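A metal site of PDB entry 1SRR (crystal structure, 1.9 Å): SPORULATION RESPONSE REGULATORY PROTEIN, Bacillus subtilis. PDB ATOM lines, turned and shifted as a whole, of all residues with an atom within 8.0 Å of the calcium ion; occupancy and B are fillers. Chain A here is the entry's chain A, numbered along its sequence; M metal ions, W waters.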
ATOM      1  N   VAL A   9      -9.396  32.008   3.694  1.00  0.00           N
ATOM      2  CA  VAL A   9     -10.640  31.982   4.379  1.00  0.00           C
ATOM      3  C   VAL A   9     -10.454  31.649   5.830  1.00  0.00           C
ATOM      4  O   VAL A   9     -10.076  30.537   6.170  1.00  0.00           O
ATOM      5  CB  VAL A   9     -11.583  30.975   3.747  1.00  0.00           C
ATOM      6  CG1 VAL A   9     -13.003  31.168   4.286  1.00  0.00           C
ATOM      7  CG2 VAL A   9     -11.529  31.052   2.194  1.00  0.00           C
ATOM      8  N   ASP A  10     -10.738  32.604   6.701  1.00  0.00           N
ATOM      9  CA  ASP A  10     -10.604  32.348   8.111  1.00  0.00           C
ATOM     10  C   ASP A  10     -11.414  33.353   8.855  1.00  0.00           C
ATOM     11  O   ASP A  10     -11.350  34.530   8.520  1.00  0.00           O
ATOM     12  CB  ASP A  10      -9.164  32.526   8.582  1.00  0.00           C
ATOM     13  CG  ASP A  10      -8.828  31.722   9.800  1.00  0.00           C
ATOM     14  OD1 ASP A  10      -9.385  32.177  10.928  1.00  0.00           O
ATOM     15  OD2 ASP A  10      -8.125  30.755   9.746  1.00  0.00           O
ATOM     16  N   ASP A  11     -12.119  32.862   9.872  1.00  0.00           N
ATOM     17  CA  ASP A  11     -12.963  33.701  10.700  1.00  0.00           C
ATOM     18  C   ASP A  11     -12.281  34.672  11.603  1.00  0.00           C
ATOM     19  O   ASP A  11     -12.903  35.632  12.038  1.00  0.00           O
ATOM     20  CB  ASP A  11     -14.127  33.011  11.400  1.00  0.00           C
ATOM     21  CG  ASP A  11     -13.690  32.076  12.474  1.00  0.00           C
ATOM     22  OD1 ASP A  11     -12.691  31.326  12.100  1.00  0.00           O
ATOM     23  OD2 ASP A  11     -14.254  31.969  13.541  1.00  0.00           O
ATOM     24  N   GLN A  12     -10.993  34.429  11.877  1.00  0.00           N
ATOM     25  CA  GLN A  12     -10.144  35.237  12.763  1.00  0.00           C
ATOM     26  C   GLN A  12      -9.186  36.229  12.061  1.00  0.00           C
ATOM     27  O   GLN A  12      -8.210  35.824  11.431  1.00  0.00           O
ATOM     28  CB  GLN A  12      -9.371  34.280  13.717  1.00  0.00           C
ATOM     29  CG  GLN A  12     -10.266  33.660  14.809  1.00  0.00           C
ATOM     30  CD  GLN A  12      -9.740  32.419  15.525  1.00  0.00           C
ATOM     31  OE1 GLN A  12      -9.930  32.289  16.750  1.00  0.00           O
ATOM     32  NE2 GLN A  12      -9.079  31.531  14.782  1.00  0.00           N
ATOM     33  N   ILE A  15      -5.095  35.907  12.645  1.00  0.00           N
ATOM     34  CA  ILE A  15      -4.451  34.803  11.926  1.00  0.00           C
ATOM     35  C   ILE A  15      -4.596  34.922  10.440  1.00  0.00           C
ATOM     36  O   ILE A  15      -3.640  34.644   9.679  1.00  0.00           O
ATOM     37  CB  ILE A  15      -4.975  33.474  12.441  1.00  0.00           C
ATOM     38  CG1 ILE A  15      -4.513  32.302  11.570  1.00  0.00           C
ATOM     39  CG2 ILE A  15      -6.481  33.554  12.439  1.00  0.00           C
ATOM     40  CD1 ILE A  15      -4.330  31.009  12.343  1.00  0.00           C
ATOM     41  N   ALA A  34     -13.930  35.992   5.447  1.00  0.00           N
ATOM     42  CA  ALA A  34     -14.198  35.625   6.856  1.00  0.00           C
ATOM     43  C   ALA A  34     -15.323  34.585   7.056  1.00  0.00           C
ATOM     44  O   ALA A  34     -15.688  34.167   8.156  1.00  0.00           O
ATOM     45  CB  ALA A  34     -14.518  36.933   7.600  1.00  0.00           C
ATOM     46  N   ASP A  54     -10.395  27.519   6.283  1.00  0.00           N
ATOM     47  CA  ASP A  54     -10.638  27.301   7.730  1.00  0.00           C
ATOM     48  C   ASP A  54     -11.945  26.521   7.794  1.00  0.00           C
ATOM     49  O   ASP A  54     -12.992  26.970   7.299  1.00  0.00           O
ATOM     50  CB  ASP A  54     -10.775  28.655   8.456  1.00  0.00           C
ATOM     51  CG  ASP A  54     -11.055  28.570   9.937  1.00  0.00           C
ATOM     52  OD1 ASP A  54     -11.071  27.331  10.399  1.00  0.00           O
ATOM     53  OD2 ASP A  54     -11.235  29.536  10.627  1.00  0.00           O
ATOM     54  N   MET A  55     -11.914  25.312   8.335  1.00  0.00           N
ATOM     55  CA  MET A  55     -13.152  24.554   8.328  1.00  0.00           C
ATOM     56  C   MET A  55     -13.986  24.832   9.577  1.00  0.00           C
ATOM     57  O   MET A  55     -15.104  24.323   9.756  1.00  0.00           O
ATOM     58  CB  MET A  55     -12.894  23.054   8.223  1.00  0.00           C
ATOM     59  CG  MET A  55     -12.040  22.721   7.080  1.00  0.00           C
ATOM     60  SD  MET A  55     -12.960  22.940   5.563  1.00  0.00           S
ATOM     61  CE  MET A  55     -13.439  21.242   5.179  1.00  0.00           C
ATOM     62  N   LYS A  56     -13.421  25.621  10.460  1.00  0.00           N
ATOM     63  CA  LYS A  56     -14.170  25.917  11.663  1.00  0.00           C
ATOM     64  C   LYS A  56     -14.612  27.360  11.686  1.00  0.00           C
ATOM     65  O   LYS A  56     -13.926  28.252  12.220  1.00  0.00           O
ATOM     66  CB  LYS A  56     -13.484  25.452  12.941  1.00  0.00           C
ATOM     67  CG  LYS A  56     -14.181  25.818  14.243  1.00  0.00           C
ATOM     68  CD  LYS A  56     -13.207  25.747  15.427  1.00  0.00           C
ATOM     69  CE  LYS A  56     -13.832  25.790  16.815  1.00  0.00           C
ATOM     70  NZ  LYS A  56     -12.826  25.639  17.898  1.00  0.00           N
ATOM     71  N   ILE A  57     -15.760  27.540  11.056  1.00  0.00           N
ATOM     72  CA  ILE A  57     -16.397  28.816  10.957  1.00  0.00           C
ATOM     73  C   ILE A  57     -17.856  28.577  11.294  1.00  0.00           C
ATOM     74  O   ILE A  57     -18.542  27.732  10.697  1.00  0.00           O
ATOM     75  CB  ILE A  57     -16.178  29.572   9.617  1.00  0.00           C
ATOM     76  CG1 ILE A  57     -14.673  29.848   9.415  1.00  0.00           C
ATOM     77  CG2 ILE A  57     -17.001  30.879   9.633  1.00  0.00           C
ATOM     78  CD1 ILE A  57     -14.266  30.520   8.107  1.00  0.00           C
ATOM     79  N   PRO A  58     -18.291  29.340  12.277  1.00  0.00           N
ATOM     80  CA  PRO A  58     -19.631  29.277  12.797  1.00  0.00           C
ATOM     81  C   PRO A  58     -20.699  29.443  11.791  1.00  0.00           C
ATOM     82  O   PRO A  58     -20.794  30.473  11.112  1.00  0.00           O
ATOM     83  CB  PRO A  58     -19.727  30.333  13.894  1.00  0.00           C
ATOM     84  CG  PRO A  58     -18.285  30.617  14.271  1.00  0.00           C
ATOM     85  CD  PRO A  58     -17.418  30.200  13.093  1.00  0.00           C
ATOM     86  N   MET A  60     -20.887  27.822   9.288  1.00  0.00           N
ATOM     87  CA  MET A  60     -20.224  27.213   8.163  1.00  0.00           C
ATOM     88  C   MET A  60     -19.944  25.675   8.129  1.00  0.00           C
ATOM     89  O   MET A  60     -19.341  25.091   9.030  1.00  0.00           O
ATOM     90  CB  MET A  60     -18.985  28.012   7.761  1.00  0.00           C
ATOM     91  CG  MET A  60     -18.549  27.612   6.360  1.00  0.00           C
ATOM     92  SD  MET A  60     -16.981  28.333   5.852  1.00  0.00           S
ATOM     93  CE  MET A  60     -15.826  27.150   6.590  1.00  0.00           C
ATOM     94  N   MET A  81      -7.886  23.815   6.669  1.00  0.00           N
ATOM     95  CA  MET A  81      -7.269  24.024   7.932  1.00  0.00           C
ATOM     96  C   MET A  81      -8.200  23.460   8.960  1.00  0.00           C
ATOM     97  O   MET A  81      -9.336  23.868   9.127  1.00  0.00           O
ATOM     98  CB  MET A  81      -6.894  25.495   8.112  1.00  0.00           C
ATOM     99  CG  MET A  81      -6.240  25.915   6.805  1.00  0.00           C
ATOM    100  SD  MET A  81      -5.572  27.561   6.933  1.00  0.00           S
ATOM    101  CE  MET A  81      -7.005  28.544   7.441  1.00  0.00           C
ATOM    102  N   ALA A  83      -8.970  21.933  12.912  1.00  0.00           N
ATOM    103  CA  ALA A  83      -8.706  22.323  14.274  1.00  0.00           C
ATOM    104  C   ALA A  83      -8.286  21.099  14.920  1.00  0.00           C
ATOM    105  O   ALA A  83      -9.117  20.367  15.490  1.00  0.00           O
ATOM    106  CB  ALA A  83      -9.953  22.832  14.974  1.00  0.00           C
ATOM    107  N   LYS A 104      -4.335  23.678  13.108  1.00  0.00           N
ATOM    108  CA  LYS A 104      -3.929  24.838  13.837  1.00  0.00           C
ATOM    109  C   LYS A 104      -3.807  24.406  15.292  1.00  0.00           C
ATOM    110  O   LYS A 104      -4.496  23.510  15.753  1.00  0.00           O
ATOM    111  CB  LYS A 104      -4.922  25.946  13.699  1.00  0.00           C
ATOM    112  CG  LYS A 104      -5.258  26.170  12.242  1.00  0.00           C
ATOM    113  CD  LYS A 104      -5.865  27.537  12.013  1.00  0.00           C
ATOM    114  CE  LYS A 104      -7.378  27.491  12.065  1.00  0.00           C
ATOM    115  NZ  LYS A 104      -8.011  28.817  11.976  1.00  0.00           N
HETATM  116 CA    CA M   1     -12.121  29.480  12.781  1.00  0.00          CA
HETATM  117  O   HOH W   1     -12.049  29.484  15.212  1.00  0.00           O
HETATM  118  O   HOH W   2     -10.366  30.624  12.760  1.00  0.00           O
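The side-chain carboxylate of Asp 54 is in salt-bridge range of the side-chain amino group of Lys 104 (3.7 Å). The backbone NH (N) of Asp 54 lies within hydrogen-bond range of the backbone carbonyl oxygen (O) of Val 9 (3.0 Å).
The calcium ion is bound by OD1 of Asp 11 (2.0 Å), water W2 (2.1 Å), O of Lys 56 (2.3 Å), OD2 of Asp 54 (2.3 Å) and water W1 (2.4 Å). The calcium ion has five donor atoms within binding distance.
Within 4 Å of the calcium ion: Asp 11, Asp 54 and Lys 56. The nearest printed residue that does not touch the calcium ion is Gln 12 (4.2 Å).
Water W2 lies within hydrogen-bond range of the side-chain amide nitrogen of Gln 12, the side-chain carboxylate of Asp 10 and the side-chain amino group of Lys 104.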
